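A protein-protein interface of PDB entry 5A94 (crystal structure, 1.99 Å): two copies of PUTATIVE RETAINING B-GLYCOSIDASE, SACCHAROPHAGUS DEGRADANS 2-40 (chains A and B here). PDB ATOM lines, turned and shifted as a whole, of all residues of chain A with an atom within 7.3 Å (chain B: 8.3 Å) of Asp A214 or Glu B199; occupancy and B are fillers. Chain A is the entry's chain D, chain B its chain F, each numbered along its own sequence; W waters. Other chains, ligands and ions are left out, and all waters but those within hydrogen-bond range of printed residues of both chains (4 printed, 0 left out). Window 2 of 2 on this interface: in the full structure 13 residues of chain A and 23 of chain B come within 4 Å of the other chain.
No position is printed for both chains.
Water W4 bridges the backbone carbonyl oxygen (O) of Gly B194 (2.5 Å) and the backbone carbonyl oxygen (O) of Ala A218 (3.1 Å). Water W1 bridges O of Met A215 and O of Thr B196. Water W2 lies within hydrogen-bond range of OD2 of Asp A214 (2.8 Å) and OE1 of Glu B199 (2.9 Å). Water W3 lies within hydrogen-bond range of the backbone carbonyl oxygen (O) of Thr B149 (2.8 Å) and the guanidinium group (NE) of Arg A165 (3.1 Å).
The guanidinium group (NH1) of Arg A165 sits at hydrogen-bond distance from the side-chain sulfur (SD) of Met A215, 3.5 Å away. The side-chain amide oxygen (OD1) of Asn B195 is in hydrogen-bond range of the side-chain hydroxyl (OG1) of Thr B192, 2.7 Å away. The backbone carbonyl oxygen of Thr B192 is in hydrogen-bond range of the side-chain hydroxyl of Thr B196, at 3.4 Å. The side-chain amide oxygen of Asn B195 lies close to the backbone carbonyl oxygen of Gly B198, 3.1 Å away. OE2 of Glu B199 lies within hydrogen-bond range of ND2 of Asn B195 (3.4 Å). N of Arg B200 lies within hydrogen-bond range of OD1 of Asn B195 (3.1 Å).
Of chain B, only Glu B199 (3.7 Å) comes within 4 Å of Asp A214. Of the printed residues of chain A, Thr B149 touches Arg A165 (3.8 Å). Thr B192 touches none of the printed residues of chain A. Printed residues of chain A within 4 Å of Asn B195: Ala A218. The nearest residue of chain A that does not touch Glu B199 is Met A215 (5.5 Å). The nearest printed residue of chain A that does not touch Asn B195 is Met A215 (4.02 Å).
Arg A165 touches Thr B149. Asp A214 touches Glu B199 (CB to OE2, 3.7 Å). Met A215 touches Thr B196. CB of Ala A218 touches O of Gly B194, at 3.7 Å. Asn B195 touches Ala A218 (O to CB, 3.4 Å). Ala A218 touches Thr B196.
Hydrophobic or aromatic side chains of chain A that line the printed part of chain B: Met A215 and Ala A218. Of the 17 printed residues of chain B, 5 touch a printed residue of chain A. Printed residues of chain B that touch a printed residue of chain A: Thr B149, Gly B194, Asn B195, Thr B196 and Glu B199. Among the printed residues, no Asp or Glu carboxylate lies within 4 Å of a Lys or Arg side-chain nitrogen of the other chain.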
ATOM      1  N   ARG A 165     -29.121   2.100  13.452  1.00  0.00           N
ATOM      2  CA  ARG A 165     -29.755   0.782  13.418  1.00  0.00           C
ATOM      3  C   ARG A 165     -31.052   0.808  12.612  1.00  0.00           C
ATOM      4  O   ARG A 165     -31.303  -0.085  11.798  1.00  0.00           O
ATOM      5  CB  ARG A 165     -30.085   0.289  14.822  1.00  0.00           C
ATOM      6  CG  ARG A 165     -28.906  -0.114  15.666  1.00  0.00           C
ATOM      7  CD  ARG A 165     -29.398  -0.663  16.990  1.00  0.00           C
ATOM      8  NE  ARG A 165     -28.325  -0.963  17.937  1.00  0.00           N
ATOM      9  CZ  ARG A 165     -27.551  -2.042  17.877  1.00  0.00           C
ATOM     10  NH1 ARG A 165     -27.710  -2.946  16.899  1.00  0.00           N
ATOM     11  NH2 ARG A 165     -26.607  -2.232  18.790  1.00  0.00           N
ATOM     12  N   THR A 207     -17.437  -4.556  17.772  1.00  0.00           N
ATOM     13  CA  THR A 207     -18.640  -5.140  18.349  1.00  0.00           C
ATOM     14  C   THR A 207     -19.877  -4.466  17.767  1.00  0.00           C
ATOM     15  O   THR A 207     -20.871  -5.125  17.483  1.00  0.00           O
ATOM     16  CB  THR A 207     -18.598  -5.038  19.889  1.00  0.00           C
ATOM     17  OG1 THR A 207     -17.536  -5.874  20.375  1.00  0.00           O
ATOM     18  CG2 THR A 207     -19.906  -5.470  20.528  1.00  0.00           C
ATOM     19  N   LEU A 208     -19.818  -3.146  17.581  1.00  0.00           N
ATOM     20  CA  LEU A 208     -20.978  -2.425  17.083  1.00  0.00           C
ATOM     21  C   LEU A 208     -21.230  -2.768  15.609  1.00  0.00           C
ATOM     22  O   LEU A 208     -22.371  -2.913  15.206  1.00  0.00           O
ATOM     23  CB  LEU A 208     -20.797  -0.911  17.278  1.00  0.00           C
ATOM     24  CG  LEU A 208     -21.971  -0.024  16.874  1.00  0.00           C
ATOM     25  CD1 LEU A 208     -23.255  -0.460  17.553  1.00  0.00           C
ATOM     26  CD2 LEU A 208     -21.657   1.423  17.204  1.00  0.00           C
ATOM     27  N   ASN A 209     -20.173  -2.897  14.810  1.00  0.00           N
ATOM     28  CA  ASN A 209     -20.330  -3.319  13.425  1.00  0.00           C
ATOM     29  C   ASN A 209     -20.918  -4.734  13.355  1.00  0.00           C
ATOM     30  O   ASN A 209     -21.763  -5.010  12.500  1.00  0.00           O
ATOM     31  CB  ASN A 209     -19.002  -3.290  12.649  1.00  0.00           C
ATOM     32  CG  ASN A 209     -18.666  -1.911  12.138  1.00  0.00           C
ATOM     33  OD1 ASN A 209     -18.979  -1.553  11.005  1.00  0.00           O
ATOM     34  ND2 ASN A 209     -18.076  -1.118  12.984  1.00  0.00           N
ATOM     35  N   GLU A 210     -20.470  -5.608  14.237  1.00  0.00           N
ATOM     36  CA  GLU A 210     -20.983  -6.980  14.265  1.00  0.00           C
ATOM     37  C   GLU A 210     -22.479  -6.968  14.616  1.00  0.00           C
ATOM     38  O   GLU A 210     -23.244  -7.761  14.082  1.00  0.00           O
ATOM     39  CB  GLU A 210     -20.170  -7.848  15.232  1.00  0.00           C
ATOM     40  CG  GLU A 210     -18.819  -8.236  14.661  1.00  0.00           C
ATOM     41  CD  GLU A 210     -17.846  -8.834  15.652  1.00  0.00           C
ATOM     42  OE1 GLU A 210     -18.179  -8.968  16.849  1.00  0.00           O
ATOM     43  OE2 GLU A 210     -16.736  -9.216  15.216  1.00  0.00           O
ATOM     44  N   SER A 211     -22.889  -6.049  15.491  1.00  0.00           N
ATOM     45  CA  SER A 211     -24.297  -5.908  15.858  1.00  0.00           C
ATOM     46  C   SER A 211     -25.135  -5.454  14.663  1.00  0.00           C
ATOM     47  O   SER A 211     -26.199  -6.017  14.398  1.00  0.00           O
ATOM     48  CB  SER A 211     -24.434  -4.938  17.029  1.00  0.00           C
ATOM     49  OG  SER A 211     -25.771  -4.822  17.478  1.00  0.00           O
ATOM     50  N   LEU A 212     -24.630  -4.480  13.898  1.00  0.00           N
ATOM     51  CA  LEU A 212     -25.306  -4.027  12.695  1.00  0.00           C
ATOM     52  C   LEU A 212     -25.378  -5.138  11.659  1.00  0.00           C
ATOM     53  O   LEU A 212     -26.428  -5.355  11.054  1.00  0.00           O
ATOM     54  CB  LEU A 212     -24.602  -2.804  12.076  1.00  0.00           C
ATOM     55  CG  LEU A 212     -24.681  -1.538  12.910  1.00  0.00           C
ATOM     56  CD1 LEU A 212     -23.778  -0.449  12.339  1.00  0.00           C
ATOM     57  CD2 LEU A 212     -26.110  -1.029  13.041  1.00  0.00           C
ATOM     58  N   ILE A 213     -24.268  -5.843  11.459  1.00  0.00           N
ATOM     59  CA  ILE A 213     -24.223  -6.956  10.502  1.00  0.00           C
ATOM     60  C   ILE A 213     -25.272  -8.014  10.860  1.00  0.00           C
ATOM     61  O   ILE A 213     -25.956  -8.526   9.969  1.00  0.00           O
ATOM     62  CB  ILE A 213     -22.810  -7.578  10.436  1.00  0.00           C
ATOM     63  CG1 ILE A 213     -21.834  -6.593   9.758  1.00  0.00           C
ATOM     64  CG2 ILE A 213     -22.807  -8.903   9.683  1.00  0.00           C
ATOM     65  CD1 ILE A 213     -20.371  -6.895  10.003  1.00  0.00           C
ATOM     66  N   ASP A 214     -25.384  -8.332  12.148  1.00  0.00           N
ATOM     67  CA  ASP A 214     -26.337  -9.341  12.616  1.00  0.00           C
ATOM     68  C   ASP A 214     -27.777  -8.957  12.297  1.00  0.00           C
ATOM     69  O   ASP A 214     -28.559  -9.810  11.886  1.00  0.00           O
ATOM     70  CB  ASP A 214     -26.172  -9.625  14.118  1.00  0.00           C
ATOM     71  CG  ASP A 214     -24.918 -10.417  14.433  1.00  0.00           C
ATOM     72  OD1 ASP A 214     -24.325 -11.005  13.509  1.00  0.00           O
ATOM     73  OD2 ASP A 214     -24.499 -10.408  15.611  1.00  0.00           O
ATOM     74  N   MET A 215     -28.120  -7.677  12.454  1.00  0.00           N
ATOM     75  CA  MET A 215     -29.467  -7.176  12.107  1.00  0.00           C
ATOM     76  C   MET A 215     -29.716  -7.297  10.611  1.00  0.00           C
ATOM     77  O   MET A 215     -30.815  -7.633  10.179  1.00  0.00           O
ATOM     78  CB  MET A 215     -29.620  -5.692  12.449  1.00  0.00           C
ATOM     79  CG  MET A 215     -29.722  -5.348  13.922  1.00  0.00           C
ATOM     80  SD  MET A 215     -29.806  -3.554  14.116  1.00  0.00           S
ATOM     81  CE  MET A 215     -31.466  -3.217  13.554  1.00  0.00           C
ATOM     82  N   ILE A 216     -28.695  -7.008   9.820  1.00  0.00           N
ATOM     83  CA  ILE A 216     -28.810  -7.083   8.363  1.00  0.00           C
ATOM     84  C   ILE A 216     -28.972  -8.532   7.904  1.00  0.00           C
ATOM     85  O   ILE A 216     -29.883  -8.854   7.139  1.00  0.00           O
ATOM     86  CB  ILE A 216     -27.596  -6.432   7.684  1.00  0.00           C
ATOM     87  CG1 ILE A 216     -27.608  -4.915   7.942  1.00  0.00           C
ATOM     88  CG2 ILE A 216     -27.617  -6.676   6.188  1.00  0.00           C
ATOM     89  CD1 ILE A 216     -26.292  -4.229   7.693  1.00  0.00           C
ATOM     90  N   TYR A 217     -28.067  -9.384   8.370  1.00  0.00           N
ATOM     91  CA  TYR A 217     -28.050 -10.782   7.980  1.00  0.00           C
ATOM     92  C   TYR A 217     -29.281 -11.553   8.436  1.00  0.00           C
ATOM     93  O   TYR A 217     -29.671 -12.521   7.789  1.00  0.00           O
ATOM     94  CB  TYR A 217     -26.780 -11.465   8.485  1.00  0.00           C
ATOM     95  CG  TYR A 217     -25.524 -11.221   7.653  1.00  0.00           C
ATOM     96  CD1 TYR A 217     -25.569 -10.564   6.425  1.00  0.00           C
ATOM     97  CD2 TYR A 217     -24.307 -11.764   8.044  1.00  0.00           C
ATOM     98  CE1 TYR A 217     -24.422 -10.403   5.647  1.00  0.00           C
ATOM     99  CE2 TYR A 217     -23.162 -11.611   7.259  1.00  0.00           C
ATOM    100  CZ  TYR A 217     -23.225 -10.919   6.068  1.00  0.00           C
ATOM    101  OH  TYR A 217     -22.082 -10.754   5.290  1.00  0.00           O
ATOM    102  N   ALA A 218     -29.883 -11.124   9.540  1.00  0.00           N
ATOM    103  CA  ALA A 218     -31.163 -11.646   9.977  1.00  0.00           C
ATOM    104  C   ALA A 218     -32.278 -11.422   8.943  1.00  0.00           C
ATOM    105  O   ALA A 218     -33.202 -12.216   8.872  1.00  0.00           O
ATOM    106  CB  ALA A 218     -31.564 -11.017  11.301  1.00  0.00           C
ATOM    107  N   SER A 219     -32.185 -10.331   8.177  1.00  0.00           N
ATOM    108  CA  SER A 219     -33.217  -9.897   7.227  1.00  0.00           C
ATOM    109  C   SER A 219     -32.837 -10.170   5.757  1.00  0.00           C
ATOM    110  O   SER A 219     -33.707 -10.441   4.924  1.00  0.00           O
ATOM    111  CB  SER A 219     -33.452  -8.390   7.456  1.00  0.00           C
ATOM    112  OG  SER A 219     -34.708  -7.894   6.999  1.00  0.00           O
ATOM    113  N   ASP A 220     -31.541 -10.113   5.426  1.00  0.00           N
ATOM    114  CA  ASP A 220     -31.076 -10.399   4.057  1.00  0.00           C
ATOM    115  C   ASP A 220     -29.612 -10.861   4.041  1.00  0.00           C
ATOM    116  O   ASP A 220     -28.702 -10.068   4.269  1.00  0.00           O
ATOM    117  CB  ASP A 220     -31.238  -9.154   3.166  1.00  0.00           C
ATOM    118  CG  ASP A 220     -30.973  -9.444   1.677  1.00  0.00           C
ATOM    119  OD1 ASP A 220     -30.481 -10.548   1.345  1.00  0.00           O
ATOM    120  OD2 ASP A 220     -31.205  -8.536   0.855  1.00  0.00           O
ATOM    121  N   PRO A 225     -21.998  -6.335   3.629  1.00  0.00           N
ATOM    122  CA  PRO A 225     -21.668  -5.229   4.503  1.00  0.00           C
ATOM    123  C   PRO A 225     -20.237  -4.757   4.259  1.00  0.00           C
ATOM    124  O   PRO A 225     -19.350  -5.565   3.977  1.00  0.00           O
ATOM    125  CB  PRO A 225     -21.794  -5.820   5.900  1.00  0.00           C
ATOM    126  CG  PRO A 225     -22.582  -7.086   5.734  1.00  0.00           C
ATOM    127  CD  PRO A 225     -22.178  -7.592   4.383  1.00  0.00           C
ATOM    128  N   GLU A 245     -15.795 -10.714  12.997  1.00  0.00           N
ATOM    129  CA  GLU A 245     -15.983 -12.172  13.052  1.00  0.00           C
ATOM    130  C   GLU A 245     -17.287 -12.551  12.374  1.00  0.00           C
ATOM    131  O   GLU A 245     -18.140 -13.198  12.965  1.00  0.00           O
ATOM    132  CB  GLU A 245     -15.940 -12.669  14.497  1.00  0.00           C
ATOM    133  CG  GLU A 245     -14.603 -12.381  15.171  1.00  0.00           C
ATOM    134  CD  GLU A 245     -14.557 -12.831  16.610  1.00  0.00           C
ATOM    135  OE1 GLU A 245     -14.561 -14.052  16.857  1.00  0.00           O
ATOM    136  OE2 GLU A 245     -14.496 -11.962  17.505  1.00  0.00           O
ATOM    137  N   ARG A 246     -17.409 -12.154  11.111  1.00  0.00           N
ATOM    138  CA  ARG A 246     -18.549 -12.495  10.275  1.00  0.00           C
ATOM    139  C   ARG A 246     -18.060 -12.729   8.850  1.00  0.00           C
ATOM    140  O   ARG A 246     -17.109 -12.080   8.397  1.00  0.00           O
ATOM    141  CB  ARG A 246     -19.570 -11.359  10.272  1.00  0.00           C
ATOM    142  CG  ARG A 246     -20.092 -10.951  11.649  1.00  0.00           C
ATOM    143  CD  ARG A 246     -21.045 -11.989  12.204  1.00  0.00           C
ATOM    144  NE  ARG A 246     -21.671 -11.568  13.455  1.00  0.00           N
ATOM    145  CZ  ARG A 246     -21.120 -11.649  14.664  1.00  0.00           C
ATOM    146  NH1 ARG A 246     -19.880 -12.108  14.834  1.00  0.00           N
ATOM    147  NH2 ARG A 246     -21.805 -11.235  15.718  1.00  0.00           N
ATOM    148  N   TYR B 146     -37.431  -4.600  20.954  1.00  0.00           N
ATOM    149  CA  TYR B 146     -36.284  -4.853  21.816  1.00  0.00           C
ATOM    150  C   TYR B 146     -35.747  -3.542  22.409  1.00  0.00           C
ATOM    151  O   TYR B 146     -35.002  -2.793  21.742  1.00  0.00           O
ATOM    152  CB  TYR B 146     -35.208  -5.615  21.040  1.00  0.00           C
ATOM    153  CG  TYR B 146     -34.248  -6.352  21.957  1.00  0.00           C
ATOM    154  CD1 TYR B 146     -34.716  -7.303  22.847  1.00  0.00           C
ATOM    155  CD2 TYR B 146     -32.877  -6.137  21.886  1.00  0.00           C
ATOM    156  CE1 TYR B 146     -33.858  -7.998  23.679  1.00  0.00           C
ATOM    157  CE2 TYR B 146     -32.010  -6.835  22.715  1.00  0.00           C
ATOM    158  CZ  TYR B 146     -32.519  -7.774  23.607  1.00  0.00           C
ATOM    159  OH  TYR B 146     -31.681  -8.447  24.461  1.00  0.00           O
ATOM    160  N   PRO B 148     -33.390  -2.879  24.701  1.00  0.00           N
ATOM    161  CA  PRO B 148     -31.938  -2.658  24.740  1.00  0.00           C
ATOM    162  C   PRO B 148     -31.304  -2.047  23.481  1.00  0.00           C
ATOM    163  O   PRO B 148     -30.344  -1.317  23.608  1.00  0.00           O
ATOM    164  CB  PRO B 148     -31.379  -4.062  24.974  1.00  0.00           C
ATOM    165  CG  PRO B 148     -32.465  -4.729  25.753  1.00  0.00           C
ATOM    166  CD  PRO B 148     -33.732  -4.255  25.104  1.00  0.00           C
ATOM    167  N   THR B 149     -31.845  -2.336  22.295  1.00  0.00           N
ATOM    168  CA  THR B 149     -31.391  -1.686  21.070  1.00  0.00           C
ATOM    169  C   THR B 149     -32.327  -0.581  20.603  1.00  0.00           C
ATOM    170  O   THR B 149     -32.035   0.079  19.616  1.00  0.00           O
ATOM    171  CB  THR B 149     -31.243  -2.700  19.918  1.00  0.00           C
ATOM    172  OG1 THR B 149     -32.480  -3.384  19.733  1.00  0.00           O
ATOM    173  CG2 THR B 149     -30.119  -3.688  20.204  1.00  0.00           C
ATOM    174  N   THR B 191     -39.578  -8.615  21.921  1.00  0.00           N
ATOM    175  CA  THR B 191     -39.276  -9.465  20.769  1.00  0.00           C
ATOM    176  C   THR B 191     -38.147  -8.823  19.962  1.00  0.00           C
ATOM    177  O   THR B 191     -38.012  -7.593  19.925  1.00  0.00           O
ATOM    178  CB  THR B 191     -40.507  -9.655  19.865  1.00  0.00           C
ATOM    179  OG1 THR B 191     -40.163 -10.474  18.749  1.00  0.00           O
ATOM    180  CG2 THR B 191     -41.041  -8.304  19.357  1.00  0.00           C
ATOM    181  N   THR B 192     -37.339  -9.655  19.312  1.00  0.00           N
ATOM    182  CA  THR B 192     -36.375  -9.165  18.339  1.00  0.00           C
ATOM    183  C   THR B 192     -36.816  -9.438  16.889  1.00  0.00           C
ATOM    184  O   THR B 192     -36.036  -9.208  15.941  1.00  0.00           O
ATOM    185  CB  THR B 192     -34.987  -9.802  18.541  1.00  0.00           C
ATOM    186  OG1 THR B 192     -35.091 -11.227  18.389  1.00  0.00           O
ATOM    187  CG2 THR B 192     -34.426  -9.451  19.916  1.00  0.00           C
ATOM    188  N   GLY B 194     -37.168 -12.310  15.094  1.00  0.00           N
ATOM    189  CA  GLY B 194     -36.160 -13.164  14.485  1.00  0.00           C
ATOM    190  C   GLY B 194     -34.772 -12.537  14.447  1.00  0.00           C
ATOM    191  O   GLY B 194     -33.990 -12.781  13.523  1.00  0.00           O
ATOM    192  N   ASN B 195     -34.453 -11.780  15.494  1.00  0.00           N
ATOM    193  CA  ASN B 195     -33.185 -11.066  15.614  1.00  0.00           C
ATOM    194  C   ASN B 195     -32.940 -10.004  14.527  1.00  0.00           C
ATOM    195  O   ASN B 195     -31.813  -9.555  14.341  1.00  0.00           O
ATOM    196  CB  ASN B 195     -32.002 -12.039  15.746  1.00  0.00           C
ATOM    197  CG  ASN B 195     -31.879 -12.620  17.153  1.00  0.00           C
ATOM    198  OD1 ASN B 195     -32.593 -12.215  18.097  1.00  0.00           O
ATOM    199  ND2 ASN B 195     -30.954 -13.552  17.312  1.00  0.00           N
ATOM    200  N   THR B 196     -34.005  -9.563  13.869  1.00  0.00           N
ATOM    201  CA  THR B 196     -33.934  -8.413  12.981  1.00  0.00           C
ATOM    202  C   THR B 196     -33.855  -7.074  13.738  1.00  0.00           C
ATOM    203  O   THR B 196     -33.396  -6.068  13.172  1.00  0.00           O
ATOM    204  CB  THR B 196     -35.127  -8.350  12.002  1.00  0.00           C
ATOM    205  OG1 THR B 196     -36.357  -8.264  12.736  1.00  0.00           O
ATOM    206  CG2 THR B 196     -35.135  -9.545  11.078  1.00  0.00           C
ATOM    207  N   LEU B 197     -34.303  -7.055  15.004  1.00  0.00           N
ATOM    208  CA  LEU B 197     -34.267  -5.838  15.825  1.00  0.00           C
ATOM    209  C   LEU B 197     -33.039  -5.734  16.722  1.00  0.00           C
ATOM    210  O   LEU B 197     -32.804  -4.691  17.358  1.00  0.00           O
ATOM    211  CB  LEU B 197     -35.524  -5.735  16.685  1.00  0.00           C
ATOM    212  CG  LEU B 197     -36.854  -5.775  15.946  1.00  0.00           C
ATOM    213  CD1 LEU B 197     -38.005  -5.540  16.904  1.00  0.00           C
ATOM    214  CD2 LEU B 197     -36.886  -4.738  14.831  1.00  0.00           C
ATOM    215  N   GLY B 198     -32.255  -6.807  16.783  1.00  0.00           N
ATOM    216  CA  GLY B 198     -31.168  -6.941  17.749  1.00  0.00           C
ATOM    217  C   GLY B 198     -30.976  -8.419  18.077  1.00  0.00           C
ATOM    218  O   GLY B 198     -31.730  -9.267  17.578  1.00  0.00           O
ATOM    219  N   GLU B 199     -29.962  -8.732  18.886  1.00  0.00           N
ATOM    220  CA  GLU B 199     -29.715 -10.116  19.334  1.00  0.00           C
ATOM    221  C   GLU B 199     -30.379 -10.328  20.686  1.00  0.00           C
ATOM    222  O   GLU B 199     -29.981  -9.710  21.678  1.00  0.00           O
ATOM    223  CB  GLU B 199     -28.215 -10.373  19.458  1.00  0.00           C
ATOM    224  CG  GLU B 199     -27.490 -10.466  18.127  1.00  0.00           C
ATOM    225  CD  GLU B 199     -27.853 -11.731  17.376  1.00  0.00           C
ATOM    226  OE1 GLU B 199     -27.600 -12.835  17.914  1.00  0.00           O
ATOM    227  OE2 GLU B 199     -28.389 -11.624  16.249  1.00  0.00           O
ATOM    228  N   ARG B 200     -31.408 -11.171  20.743  1.00  0.00           N
ATOM    229  CA  ARG B 200     -32.095 -11.365  22.016  1.00  0.00           C
ATOM    230  C   ARG B 200     -31.064 -11.879  23.020  1.00  0.00           C
ATOM    231  O   ARG B 200     -30.241 -12.727  22.702  1.00  0.00           O
ATOM    232  CB  ARG B 200     -33.300 -12.294  21.889  1.00  0.00           C
ATOM    233  CG  ARG B 200     -32.991 -13.742  21.589  1.00  0.00           C
ATOM    234  CD  ARG B 200     -34.274 -14.551  21.469  1.00  0.00           C
ATOM    235  NE  ARG B 200     -35.048 -14.226  20.263  1.00  0.00           N
ATOM    236  CZ  ARG B 200     -34.780 -14.667  19.037  1.00  0.00           C
ATOM    237  NH1 ARG B 200     -33.724 -15.437  18.802  1.00  0.00           N
ATOM    238  NH2 ARG B 200     -35.551 -14.302  18.020  1.00  0.00           N
ATOM    239  N   ASN B 201     -31.088 -11.322  24.220  1.00  0.00           N
ATOM    240  CA  ASN B 201     -30.173 -11.748  25.271  1.00  0.00           C
ATOM    241  C   ASN B 201     -30.846 -11.589  26.627  1.00  0.00           C
ATOM    242  O   ASN B 201     -31.066 -10.469  27.091  1.00  0.00           O
ATOM    243  CB  ASN B 201     -28.897 -10.913  25.239  1.00  0.00           C
ATOM    244  CG  ASN B 201     -27.906 -11.324  26.312  1.00  0.00           C
ATOM    245  OD1 ASN B 201     -27.815 -10.697  27.370  1.00  0.00           O
ATOM    246  ND2 ASN B 201     -27.157 -12.393  26.047  1.00  0.00           N
ATOM    247  N   TRP B 202     -31.151 -12.712  27.269  1.00  0.00           N
ATOM    248  CA  TRP B 202     -31.879 -12.679  28.521  1.00  0.00           C
ATOM    249  C   TRP B 202     -31.156 -11.875  29.602  1.00  0.00           C
ATOM    250  O   TRP B 202     -31.793 -11.147  30.349  1.00  0.00           O
ATOM    251  CB  TRP B 202     -32.203 -14.100  29.041  1.00  0.00           C
ATOM    252  CG  TRP B 202     -32.869 -14.050  30.360  1.00  0.00           C
ATOM    253  CD1 TRP B 202     -32.321 -14.359  31.576  1.00  0.00           C
ATOM    254  CD2 TRP B 202     -34.195 -13.621  30.617  1.00  0.00           C
ATOM    255  NE1 TRP B 202     -33.232 -14.137  32.569  1.00  0.00           N
ATOM    256  CE2 TRP B 202     -34.396 -13.688  32.007  1.00  0.00           C
ATOM    257  CE3 TRP B 202     -35.239 -13.171  29.805  1.00  0.00           C
ATOM    258  CZ2 TRP B 202     -35.615 -13.352  32.605  1.00  0.00           C
ATOM    259  CZ3 TRP B 202     -36.445 -12.822  30.400  1.00  0.00           C
ATOM    260  CH2 TRP B 202     -36.623 -12.918  31.784  1.00  0.00           C
ATOM    261  N   GLU B 204     -29.135  -9.364  29.549  1.00  0.00           N
ATOM    262  CA  GLU B 204     -29.270  -7.913  29.384  1.00  0.00           C
ATOM    263  C   GLU B 204     -30.705  -7.423  29.641  1.00  0.00           C
ATOM    264  O   GLU B 204     -30.882  -6.413  30.275  1.00  0.00           O
ATOM    265  CB  GLU B 204     -28.674  -7.404  28.086  1.00  0.00           C
ATOM    266  CG  GLU B 204     -29.590  -7.268  26.929  1.00  0.00           C
ATOM    267  CD  GLU B 204     -28.898  -6.737  25.699  1.00  0.00           C
ATOM    268  OE1 GLU B 204     -28.038  -5.873  25.795  1.00  0.00           O
ATOM    269  OE2 GLU B 204     -29.261  -7.140  24.619  1.00  0.00           O
ATOM    270  N   TRP B 205     -31.701  -8.189  29.213  1.00  0.00           N
ATOM    271  CA  TRP B 205     -33.112  -7.873  29.428  1.00  0.00           C
ATOM    272  C   TRP B 205     -33.484  -8.001  30.910  1.00  0.00           C
ATOM    273  O   TRP B 205     -34.204  -7.167  31.460  1.00  0.00           O
ATOM    274  CB  TRP B 205     -34.003  -8.767  28.548  1.00  0.00           C
ATOM    275  CG  TRP B 205     -35.452  -8.472  28.647  1.00  0.00           C
ATOM    276  CD1 TRP B 205     -36.438  -9.349  28.957  1.00  0.00           C
ATOM    277  CD2 TRP B 205     -36.084  -7.196  28.483  1.00  0.00           C
ATOM    278  NE1 TRP B 205     -37.655  -8.713  28.963  1.00  0.00           N
ATOM    279  CE2 TRP B 205     -37.460  -7.384  28.687  1.00  0.00           C
ATOM    280  CE3 TRP B 205     -35.616  -5.908  28.184  1.00  0.00           C
ATOM    281  CZ2 TRP B 205     -38.373  -6.347  28.597  1.00  0.00           C
ATOM    282  CZ3 TRP B 205     -36.513  -4.883  28.111  1.00  0.00           C
ATOM    283  CH2 TRP B 205     -37.883  -5.102  28.297  1.00  0.00           C
ATOM    284  N   PHE B 230     -39.278 -13.245  26.048  1.00  0.00           N
ATOM    285  CA  PHE B 230     -39.165 -13.034  24.618  1.00  0.00           C
ATOM    286  C   PHE B 230     -40.282 -13.699  23.796  1.00  0.00           C
ATOM    287  O   PHE B 230     -41.247 -14.262  24.360  1.00  0.00           O
ATOM    288  CB  PHE B 230     -37.779 -13.463  24.136  1.00  0.00           C
ATOM    289  CG  PHE B 230     -36.638 -12.717  24.787  1.00  0.00           C
ATOM    290  CD1 PHE B 230     -36.708 -11.345  25.036  1.00  0.00           C
ATOM    291  CD2 PHE B 230     -35.472 -13.387  25.111  1.00  0.00           C
ATOM    292  CE1 PHE B 230     -35.644 -10.673  25.639  1.00  0.00           C
ATOM    293  CE2 PHE B 230     -34.404 -12.730  25.678  1.00  0.00           C
ATOM    294  CZ  PHE B 230     -34.480 -11.370  25.942  1.00  0.00           C
HETATM  295  O   HOH W   1     -32.938  -5.788  10.358  1.00  0.00           O
HETATM  296  O   HOH W   2     -25.016 -13.008  16.603  1.00  0.00           O
HETATM  297  O   HOH W   3     -29.439   1.237  19.808  1.00  0.00           O
HETATM  298  O   HOH W   4     -34.512 -13.645  11.270  1.00  0.00           O
